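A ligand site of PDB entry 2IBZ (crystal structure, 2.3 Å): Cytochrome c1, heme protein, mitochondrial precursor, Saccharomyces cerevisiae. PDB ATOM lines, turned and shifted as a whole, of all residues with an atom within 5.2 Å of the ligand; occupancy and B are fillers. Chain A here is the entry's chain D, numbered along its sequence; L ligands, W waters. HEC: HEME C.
The side-chain sulfur of Cys 40 is bonded to a carbon (CAB) of the ligand (1.8 Å). A carbon (CAC) of the ligand is covalently linked to the side-chain sulfur (SG) of Cys 43 (1.8 Å). NE2 of His 44 is bound to FE of the ligand. The side-chain sulfur of Met 164 is bound to an iron atom (FE) of the ligand. An oxygen (O2A) of the ligand lies within hydrogen-bond range of the side-chain hydroxyl (OH) of Tyr 129, at 2.6 Å. O2D of the ligand lies within hydrogen-bond range of N of Ala 163 (2.9 Å). The guanidinium group (NH1) of Arg 123 is in salt-bridge range of an oxygen (O1A) of the ligand (3.0 Å).
Merely in contact with the ligand: Val 39, Phe 157, Ile 162, Val 167, Asn 108, Pro 114, Ile 130, Pro 113, Leu 134, Leu 168, Ile 119 and Leu 194. Of the 27 residues printed, 19 come within 4 Å of the ligand. The nearest printed residue that does not touch the ligand is Leu 112 (4.05 Å).
ND1 of His 44 sits at hydrogen-bond distance from O of Pro 114, 2.8 Å away.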
ATOM      1  N   VAL A  35       4.777 -23.697   4.553  1.00  0.00           N
ATOM      2  CA  VAL A  35       3.662 -24.450   4.004  1.00  0.00           C
ATOM      3  C   VAL A  35       3.439 -23.992   2.580  1.00  0.00           C
ATOM      4  O   VAL A  35       3.199 -24.809   1.692  1.00  0.00           O
ATOM      5  CB  VAL A  35       2.382 -24.243   4.833  1.00  0.00           C
ATOM      6  CG1 VAL A  35       1.200 -24.954   4.184  1.00  0.00           C
ATOM      7  CG2 VAL A  35       2.584 -24.748   6.254  1.00  0.00           C
ATOM      8  N   VAL A  39       4.077 -26.857  -0.191  1.00  0.00           N
ATOM      9  CA  VAL A  39       2.827 -27.414  -0.698  1.00  0.00           C
ATOM     10  C   VAL A  39       2.231 -26.580  -1.844  1.00  0.00           C
ATOM     11  O   VAL A  39       2.293 -26.981  -3.018  1.00  0.00           O
ATOM     12  CB  VAL A  39       1.782 -27.559   0.435  1.00  0.00           C
ATOM     13  CG1 VAL A  39       0.608 -28.412  -0.026  1.00  0.00           C
ATOM     14  CG2 VAL A  39       2.422 -28.160   1.679  1.00  0.00           C
ATOM     15  N   CYS A  40       1.728 -25.391  -1.487  1.00  0.00           N
ATOM     16  CA  CYS A  40       1.062 -24.476  -2.421  1.00  0.00           C
ATOM     17  C   CYS A  40       1.802 -23.992  -3.657  1.00  0.00           C
ATOM     18  O   CYS A  40       1.246 -23.996  -4.751  1.00  0.00           O
ATOM     19  CB  CYS A  40       0.531 -23.270  -1.660  1.00  0.00           C
ATOM     20  SG  CYS A  40      -0.142 -23.671  -0.018  1.00  0.00           S
ATOM     21  N   ALA A  42       3.630 -25.151  -5.755  1.00  0.00           N
ATOM     22  CA  ALA A  42       3.707 -26.029  -6.916  1.00  0.00           C
ATOM     23  C   ALA A  42       2.652 -25.674  -7.969  1.00  0.00           C
ATOM     24  O   ALA A  42       2.823 -25.983  -9.155  1.00  0.00           O
ATOM     25  CB  ALA A  42       3.547 -27.474  -6.477  1.00  0.00           C
ATOM     26  N   CYS A  43       1.564 -25.034  -7.527  1.00  0.00           N
ATOM     27  CA  CYS A  43       0.485 -24.634  -8.432  1.00  0.00           C
ATOM     28  C   CYS A  43       0.098 -23.157  -8.335  1.00  0.00           C
ATOM     29  O   CYS A  43      -0.537 -22.637  -9.261  1.00  0.00           O
ATOM     30  CB  CYS A  43      -0.762 -25.464  -8.157  1.00  0.00           C
ATOM     31  SG  CYS A  43      -0.493 -27.228  -7.889  1.00  0.00           S
ATOM     32  N   HIS A  44       0.428 -22.509  -7.219  1.00  0.00           N
ATOM     33  CA  HIS A  44       0.079 -21.110  -6.968  1.00  0.00           C
ATOM     34  C   HIS A  44       1.206 -20.097  -6.992  1.00  0.00           C
ATOM     35  O   HIS A  44       2.164 -20.201  -6.210  1.00  0.00           O
ATOM     36  CB  HIS A  44      -0.613 -20.972  -5.602  1.00  0.00           C
ATOM     37  CG  HIS A  44      -2.004 -21.521  -5.550  1.00  0.00           C
ATOM     38  ND1 HIS A  44      -3.049 -21.049  -6.324  1.00  0.00           N
ATOM     39  CD2 HIS A  44      -2.525 -22.504  -4.782  1.00  0.00           C
ATOM     40  CE1 HIS A  44      -4.142 -21.767  -6.010  1.00  0.00           C
ATOM     41  NE2 HIS A  44      -3.871 -22.657  -5.078  1.00  0.00           N
ATOM     42  N   ASN A 108      -3.424 -28.515 -14.688  1.00  0.00           N
ATOM     43  CA  ASN A 108      -4.520 -28.633 -13.722  1.00  0.00           C
ATOM     44  C   ASN A 108      -5.877 -28.947 -14.312  1.00  0.00           C
ATOM     45  O   ASN A 108      -6.886 -28.372 -13.896  1.00  0.00           O
ATOM     46  CB  ASN A 108      -4.630 -27.354 -12.880  1.00  0.00           C
ATOM     47  CG  ASN A 108      -3.412 -27.121 -12.038  1.00  0.00           C
ATOM     48  OD1 ASN A 108      -3.369 -27.544 -10.886  1.00  0.00           O
ATOM     49  ND2 ASN A 108      -2.403 -26.464 -12.607  1.00  0.00           N
ATOM     50  N   ALA A 111      -7.945 -26.021 -15.340  1.00  0.00           N
ATOM     51  CA  ALA A 111      -8.293 -25.019 -14.338  1.00  0.00           C
ATOM     52  C   ALA A 111      -7.111 -24.068 -14.083  1.00  0.00           C
ATOM     53  O   ALA A 111      -5.966 -24.422 -14.346  1.00  0.00           O
ATOM     54  CB  ALA A 111      -8.717 -25.686 -13.048  1.00  0.00           C
ATOM     55  N   LEU A 112      -7.406 -22.881 -13.573  1.00  0.00           N
ATOM     56  CA  LEU A 112      -6.361 -21.900 -13.321  1.00  0.00           C
ATOM     57  C   LEU A 112      -6.226 -21.550 -11.837  1.00  0.00           C
ATOM     58  O   LEU A 112      -7.115 -20.938 -11.253  1.00  0.00           O
ATOM     59  CB  LEU A 112      -6.626 -20.646 -14.143  1.00  0.00           C
ATOM     60  CG  LEU A 112      -5.598 -19.529 -14.218  1.00  0.00           C
ATOM     61  CD1 LEU A 112      -4.301 -20.022 -14.844  1.00  0.00           C
ATOM     62  CD2 LEU A 112      -6.180 -18.374 -15.042  1.00  0.00           C
ATOM     63  N   PRO A 113      -5.134 -21.995 -11.204  1.00  0.00           N
ATOM     64  CA  PRO A 113      -4.931 -21.703  -9.786  1.00  0.00           C
ATOM     65  C   PRO A 113      -4.657 -20.199  -9.665  1.00  0.00           C
ATOM     66  O   PRO A 113      -3.694 -19.697 -10.244  1.00  0.00           O
ATOM     67  CB  PRO A 113      -3.676 -22.499  -9.438  1.00  0.00           C
ATOM     68  CG  PRO A 113      -3.627 -23.573 -10.494  1.00  0.00           C
ATOM     69  CD  PRO A 113      -4.067 -22.848 -11.731  1.00  0.00           C
ATOM     70  N   PRO A 114      -5.517 -19.456  -8.954  1.00  0.00           N
ATOM     71  CA  PRO A 114      -5.276 -18.021  -8.830  1.00  0.00           C
ATOM     72  C   PRO A 114      -4.044 -17.672  -8.022  1.00  0.00           C
ATOM     73  O   PRO A 114      -3.527 -18.484  -7.259  1.00  0.00           O
ATOM     74  CB  PRO A 114      -6.540 -17.521  -8.130  1.00  0.00           C
ATOM     75  CG  PRO A 114      -6.873 -18.653  -7.238  1.00  0.00           C
ATOM     76  CD  PRO A 114      -6.712 -19.836  -8.172  1.00  0.00           C
ATOM     77  N   LEU A 116      -2.103 -15.934  -5.106  1.00  0.00           N
ATOM     78  CA  LEU A 116      -2.574 -15.800  -3.739  1.00  0.00           C
ATOM     79  C   LEU A 116      -2.186 -14.520  -3.006  1.00  0.00           C
ATOM     80  O   LEU A 116      -2.468 -14.376  -1.806  1.00  0.00           O
ATOM     81  CB  LEU A 116      -2.134 -17.024  -2.920  1.00  0.00           C
ATOM     82  CG  LEU A 116      -2.674 -18.394  -3.361  1.00  0.00           C
ATOM     83  CD1 LEU A 116      -2.196 -19.469  -2.384  1.00  0.00           C
ATOM     84  CD2 LEU A 116      -4.197 -18.384  -3.410  1.00  0.00           C
ATOM     85  N   ILE A 119      -5.601 -13.043  -2.302  1.00  0.00           N
ATOM     86  CA  ILE A 119      -6.683 -13.990  -2.041  1.00  0.00           C
ATOM     87  C   ILE A 119      -7.505 -13.750  -0.770  1.00  0.00           C
ATOM     88  O   ILE A 119      -8.722 -13.902  -0.810  1.00  0.00           O
ATOM     89  CB  ILE A 119      -6.214 -15.487  -2.185  1.00  0.00           C
ATOM     90  CG1 ILE A 119      -7.335 -16.300  -2.854  1.00  0.00           C
ATOM     91  CG2 ILE A 119      -5.819 -16.118  -0.845  1.00  0.00           C
ATOM     92  CD1 ILE A 119      -7.548 -15.908  -4.316  1.00  0.00           C
ATOM     93  N   ARG A 123     -12.029 -12.338  -1.330  1.00  0.00           N
ATOM     94  CA  ARG A 123     -13.075 -13.309  -1.037  1.00  0.00           C
ATOM     95  C   ARG A 123     -13.833 -12.920   0.221  1.00  0.00           C
ATOM     96  O   ARG A 123     -13.210 -12.488   1.198  1.00  0.00           O
ATOM     97  CB  ARG A 123     -12.487 -14.724  -0.827  1.00  0.00           C
ATOM     98  CG  ARG A 123     -11.796 -15.379  -2.020  1.00  0.00           C
ATOM     99  CD  ARG A 123     -12.760 -15.744  -3.139  1.00  0.00           C
ATOM    100  NE  ARG A 123     -12.067 -16.479  -4.199  1.00  0.00           N
ATOM    101  CZ  ARG A 123     -11.313 -15.936  -5.154  1.00  0.00           C
ATOM    102  NH1 ARG A 123     -10.719 -16.712  -6.046  1.00  0.00           N
ATOM    103  NH2 ARG A 123     -11.166 -14.615  -5.248  1.00  0.00           N
ATOM    104  N   TYR A 129     -12.784 -17.964   5.574  1.00  0.00           N
ATOM    105  CA  TYR A 129     -13.120 -18.692   4.364  1.00  0.00           C
ATOM    106  C   TYR A 129     -11.972 -19.586   3.920  1.00  0.00           C
ATOM    107  O   TYR A 129     -12.154 -20.779   3.750  1.00  0.00           O
ATOM    108  CB  TYR A 129     -13.516 -17.732   3.225  1.00  0.00           C
ATOM    109  CG  TYR A 129     -13.627 -18.406   1.884  1.00  0.00           C
ATOM    110  CD1 TYR A 129     -14.665 -19.307   1.622  1.00  0.00           C
ATOM    111  CD2 TYR A 129     -12.671 -18.205   0.896  1.00  0.00           C
ATOM    112  CE1 TYR A 129     -14.729 -19.998   0.414  1.00  0.00           C
ATOM    113  CE2 TYR A 129     -12.735 -18.883  -0.318  1.00  0.00           C
ATOM    114  CZ  TYR A 129     -13.775 -19.785  -0.542  1.00  0.00           C
ATOM    115  OH  TYR A 129     -13.840 -20.470  -1.734  1.00  0.00           O
ATOM    116  N   ILE A 130     -10.789 -18.998   3.715  1.00  0.00           N
ATOM    117  CA  ILE A 130      -9.607 -19.736   3.260  1.00  0.00           C
ATOM    118  C   ILE A 130      -9.314 -20.933   4.175  1.00  0.00           C
ATOM    119  O   ILE A 130      -9.055 -22.043   3.696  1.00  0.00           O
ATOM    120  CB  ILE A 130      -8.355 -18.824   3.252  1.00  0.00           C
ATOM    121  CG1 ILE A 130      -8.627 -17.520   2.485  1.00  0.00           C
ATOM    122  CG2 ILE A 130      -7.176 -19.569   2.634  1.00  0.00           C
ATOM    123  CD1 ILE A 130      -8.815 -17.681   0.990  1.00  0.00           C
ATOM    124  N   LEU A 133     -12.064 -23.598   3.836  1.00  0.00           N
ATOM    125  CA  LEU A 133     -11.980 -24.300   2.557  1.00  0.00           C
ATOM    126  C   LEU A 133     -10.923 -25.409   2.632  1.00  0.00           C
ATOM    127  O   LEU A 133     -11.192 -26.551   2.264  1.00  0.00           O
ATOM    128  CB  LEU A 133     -11.612 -23.321   1.427  1.00  0.00           C
ATOM    129  CG  LEU A 133     -11.502 -23.957   0.034  1.00  0.00           C
ATOM    130  CD1 LEU A 133     -12.891 -24.141  -0.568  1.00  0.00           C
ATOM    131  CD2 LEU A 133     -10.644 -23.102  -0.883  1.00  0.00           C
ATOM    132  N   LEU A 134      -9.744 -25.061   3.134  1.00  0.00           N
ATOM    133  CA  LEU A 134      -8.623 -25.998   3.239  1.00  0.00           C
ATOM    134  C   LEU A 134      -8.832 -27.182   4.177  1.00  0.00           C
ATOM    135  O   LEU A 134      -8.255 -28.249   3.978  1.00  0.00           O
ATOM    136  CB  LEU A 134      -7.352 -25.261   3.639  1.00  0.00           C
ATOM    137  CG  LEU A 134      -6.752 -24.272   2.629  1.00  0.00           C
ATOM    138  CD1 LEU A 134      -5.659 -23.473   3.288  1.00  0.00           C
ATOM    139  CD2 LEU A 134      -6.226 -25.017   1.418  1.00  0.00           C
ATOM    140  N   PHE A 157     -17.131 -23.922  -0.886  1.00  0.00           N
ATOM    141  CA  PHE A 157     -16.976 -23.329  -2.200  1.00  0.00           C
ATOM    142  C   PHE A 157     -18.361 -23.239  -2.857  1.00  0.00           C
ATOM    143  O   PHE A 157     -19.153 -24.178  -2.760  1.00  0.00           O
ATOM    144  CB  PHE A 157     -16.069 -24.230  -3.042  1.00  0.00           C
ATOM    145  CG  PHE A 157     -15.626 -23.609  -4.338  1.00  0.00           C
ATOM    146  CD1 PHE A 157     -14.755 -22.521  -4.347  1.00  0.00           C
ATOM    147  CD2 PHE A 157     -16.070 -24.129  -5.563  1.00  0.00           C
ATOM    148  CE1 PHE A 157     -14.329 -21.948  -5.566  1.00  0.00           C
ATOM    149  CE2 PHE A 157     -15.660 -23.569  -6.772  1.00  0.00           C
ATOM    150  CZ  PHE A 157     -14.786 -22.470  -6.773  1.00  0.00           C
ATOM    151  N   SER A 161     -18.540 -27.775  -6.193  1.00  0.00           N
ATOM    152  CA  SER A 161     -17.583 -28.429  -7.070  1.00  0.00           C
ATOM    153  C   SER A 161     -16.333 -27.576  -7.341  1.00  0.00           C
ATOM    154  O   SER A 161     -16.359 -26.644  -8.151  1.00  0.00           O
ATOM    155  CB  SER A 161     -18.281 -28.819  -8.375  1.00  0.00           C
ATOM    156  OG  SER A 161     -17.363 -29.358  -9.303  1.00  0.00           O
ATOM    157  N   ILE A 162     -15.226 -27.916  -6.670  1.00  0.00           N
ATOM    158  CA  ILE A 162     -13.975 -27.179  -6.807  1.00  0.00           C
ATOM    159  C   ILE A 162     -12.885 -28.000  -7.497  1.00  0.00           C
ATOM    160  O   ILE A 162     -12.739 -29.184  -7.232  1.00  0.00           O
ATOM    161  CB  ILE A 162     -13.492 -26.699  -5.429  1.00  0.00           C
ATOM    162  CG1 ILE A 162     -12.296 -25.746  -5.585  1.00  0.00           C
ATOM    163  CG2 ILE A 162     -13.172 -27.893  -4.550  1.00  0.00           C
ATOM    164  CD1 ILE A 162     -11.867 -25.065  -4.290  1.00  0.00           C
ATOM    165  N   ALA A 163     -12.107 -27.341  -8.362  1.00  0.00           N
ATOM    166  CA  ALA A 163     -11.041 -28.008  -9.122  1.00  0.00           C
ATOM    167  C   ALA A 163      -9.746 -28.279  -8.370  1.00  0.00           C
ATOM    168  O   ALA A 163      -8.801 -28.828  -8.935  1.00  0.00           O
ATOM    169  CB  ALA A 163     -10.761 -27.232 -10.406  1.00  0.00           C
ATOM    170  N   MET A 164      -9.673 -27.873  -7.120  1.00  0.00           N
ATOM    171  CA  MET A 164      -8.490 -28.111  -6.302  1.00  0.00           C
ATOM    172  C   MET A 164      -8.854 -29.215  -5.331  1.00  0.00           C
ATOM    173  O   MET A 164      -9.868 -29.138  -4.625  1.00  0.00           O
ATOM    174  CB  MET A 164      -8.075 -26.860  -5.507  1.00  0.00           C
ATOM    175  CG  MET A 164      -6.990 -27.107  -4.473  1.00  0.00           C
ATOM    176  SD  MET A 164      -6.337 -25.626  -3.662  1.00  0.00           S
ATOM    177  CE  MET A 164      -7.607 -25.309  -2.467  1.00  0.00           C
ATOM    178  N   VAL A 167      -5.153 -30.868  -0.282  1.00  0.00           N
ATOM    179  CA  VAL A 167      -3.693 -31.001  -0.373  1.00  0.00           C
ATOM    180  C   VAL A 167      -2.984 -31.017   0.974  1.00  0.00           C
ATOM    181  O   VAL A 167      -1.782 -31.266   1.034  1.00  0.00           O
ATOM    182  CB  VAL A 167      -3.061 -29.919  -1.278  1.00  0.00           C
ATOM    183  CG1 VAL A 167      -3.651 -29.978  -2.663  1.00  0.00           C
ATOM    184  CG2 VAL A 167      -3.211 -28.524  -0.672  1.00  0.00           C
ATOM    185  N   LEU A 168      -3.702 -30.710   2.044  1.00  0.00           N
ATOM    186  CA  LEU A 168      -3.108 -30.712   3.365  1.00  0.00           C
ATOM    187  C   LEU A 168      -3.437 -32.028   4.058  1.00  0.00           C
ATOM    188  O   LEU A 168      -4.595 -32.440   4.103  1.00  0.00           O
ATOM    189  CB  LEU A 168      -3.623 -29.549   4.211  1.00  0.00           C
ATOM    190  CG  LEU A 168      -3.235 -28.143   3.778  1.00  0.00           C
ATOM    191  CD1 LEU A 168      -3.825 -27.126   4.751  1.00  0.00           C
ATOM    192  CD2 LEU A 168      -1.717 -28.012   3.720  1.00  0.00           C
ATOM    193  N   VAL A 190      -0.657 -20.979   6.922  1.00  0.00           N
ATOM    194  CA  VAL A 190      -0.600 -20.373   5.577  1.00  0.00           C
ATOM    195  C   VAL A 190      -1.581 -19.227   5.488  1.00  0.00           C
ATOM    196  O   VAL A 190      -1.304 -18.209   4.873  1.00  0.00           O
ATOM    197  CB  VAL A 190      -0.997 -21.311   4.419  1.00  0.00           C
ATOM    198  CG1 VAL A 190       0.201 -21.779   3.690  1.00  0.00           C
ATOM    199  CG2 VAL A 190      -1.896 -22.410   4.879  1.00  0.00           C
ATOM    200  N   LEU A 194      -0.891 -15.682   4.268  1.00  0.00           N
ATOM    201  CA  LEU A 194      -1.557 -15.083   3.127  1.00  0.00           C
ATOM    202  C   LEU A 194      -2.243 -13.763   3.497  1.00  0.00           C
ATOM    203  O   LEU A 194      -2.284 -12.850   2.679  1.00  0.00           O
ATOM    204  CB  LEU A 194      -2.505 -16.087   2.466  1.00  0.00           C
ATOM    205  CG  LEU A 194      -1.773 -17.290   1.830  1.00  0.00           C
ATOM    206  CD1 LEU A 194      -2.758 -18.254   1.202  1.00  0.00           C
ATOM    207  CD2 LEU A 194      -0.771 -16.814   0.784  1.00  0.00           C
HETATM  208 FE   HEC L   1      -5.075 -24.101  -4.512  1.00  0.00          FE
HETATM  209  CHA HEC L   1      -7.749 -22.592  -5.995  1.00  0.00           C
HETATM  210  CHB HEC L   1      -5.530 -22.076  -1.756  1.00  0.00           C
HETATM  211  CHC HEC L   1      -2.560 -25.734  -2.867  1.00  0.00           C
HETATM  212  CHD HEC L   1      -4.603 -26.092  -7.235  1.00  0.00           C
HETATM  213  NA  HEC L   1      -6.355 -22.603  -3.982  1.00  0.00           N
HETATM  214  C1A HEC L   1      -7.395 -22.109  -4.738  1.00  0.00           C
HETATM  215  C2A HEC L   1      -8.056 -21.044  -4.035  1.00  0.00           C
HETATM  216  C3A HEC L   1      -7.487 -20.951  -2.824  1.00  0.00           C
HETATM  217  C4A HEC L   1      -6.406 -21.897  -2.800  1.00  0.00           C
HETATM  218  CMA HEC L   1      -7.859 -20.024  -1.673  1.00  0.00           C
HETATM  219  CAA HEC L   1      -9.177 -20.206  -4.559  1.00  0.00           C
HETATM  220  CBA HEC L   1     -10.525 -20.798  -4.236  1.00  0.00           C
HETATM  221  CGA HEC L   1     -11.662 -19.834  -4.555  1.00  0.00           C
HETATM  222  O1A HEC L   1     -11.839 -19.500  -5.747  1.00  0.00           O
HETATM  223  O2A HEC L   1     -12.391 -19.430  -3.613  1.00  0.00           O
HETATM  224  NB  HEC L   1      -4.189 -23.904  -2.705  1.00  0.00           N
HETATM  225  C1B HEC L   1      -4.497 -22.995  -1.714  1.00  0.00           C
HETATM  226  C2B HEC L   1      -3.515 -23.063  -0.672  1.00  0.00           C
HETATM  227  C3B HEC L   1      -2.742 -24.132  -0.923  1.00  0.00           C
HETATM  228  C4B HEC L   1      -3.178 -24.679  -2.200  1.00  0.00           C
HETATM  229  CMB HEC L   1      -3.390 -22.106   0.495  1.00  0.00           C
HETATM  230  CAB HEC L   1      -1.587 -24.731  -0.119  1.00  0.00           C
HETATM  231  CBB HEC L   1      -2.029 -25.013   1.320  1.00  0.00           C
HETATM  232  NC  HEC L   1      -3.795 -25.585  -4.979  1.00  0.00           N
HETATM  233  C1C HEC L   1      -2.832 -26.143  -4.162  1.00  0.00           C
HETATM  234  C2C HEC L   1      -2.018 -27.043  -4.950  1.00  0.00           C
HETATM  235  C3C HEC L   1      -2.567 -27.118  -6.178  1.00  0.00           C
HETATM  236  C4C HEC L   1      -3.740 -26.285  -6.169  1.00  0.00           C
HETATM  237  CMC HEC L   1      -0.697 -27.708  -4.559  1.00  0.00           C
HETATM  238  CAC HEC L   1      -2.162 -27.759  -7.479  1.00  0.00           C
HETATM  239  CBC HEC L   1      -2.212 -29.287  -7.388  1.00  0.00           C
HETATM  240  ND  HEC L   1      -5.981 -24.293  -6.260  1.00  0.00           N
HETATM  241  C1D HEC L   1      -5.645 -25.169  -7.267  1.00  0.00           C
HETATM  242  C2D HEC L   1      -6.601 -25.054  -8.330  1.00  0.00           C
HETATM  243  C3D HEC L   1      -7.518 -24.118  -7.969  1.00  0.00           C
HETATM  244  C4D HEC L   1      -7.096 -23.617  -6.689  1.00  0.00           C
HETATM  245  CMD HEC L   1      -6.524 -25.913  -9.584  1.00  0.00           C
HETATM  246  CAD HEC L   1      -8.748 -23.677  -8.759  1.00  0.00           C
HETATM  247  CBD HEC L   1     -10.105 -23.938  -8.107  1.00  0.00           C
HETATM  248  CGD HEC L   1     -11.282 -23.782  -9.067  1.00  0.00           C
HETATM  249  O1D HEC L   1     -11.249 -22.892  -9.938  1.00  0.00           O
HETATM  250  O2D HEC L   1     -12.246 -24.550  -8.952  1.00  0.00           O
HETATM  251  O   HOH W   1     -15.321 -18.226  -4.594  1.00  0.00           O
HETATM  252  O   HOH W   2     -10.441 -20.515  -7.906  1.00  0.00           O
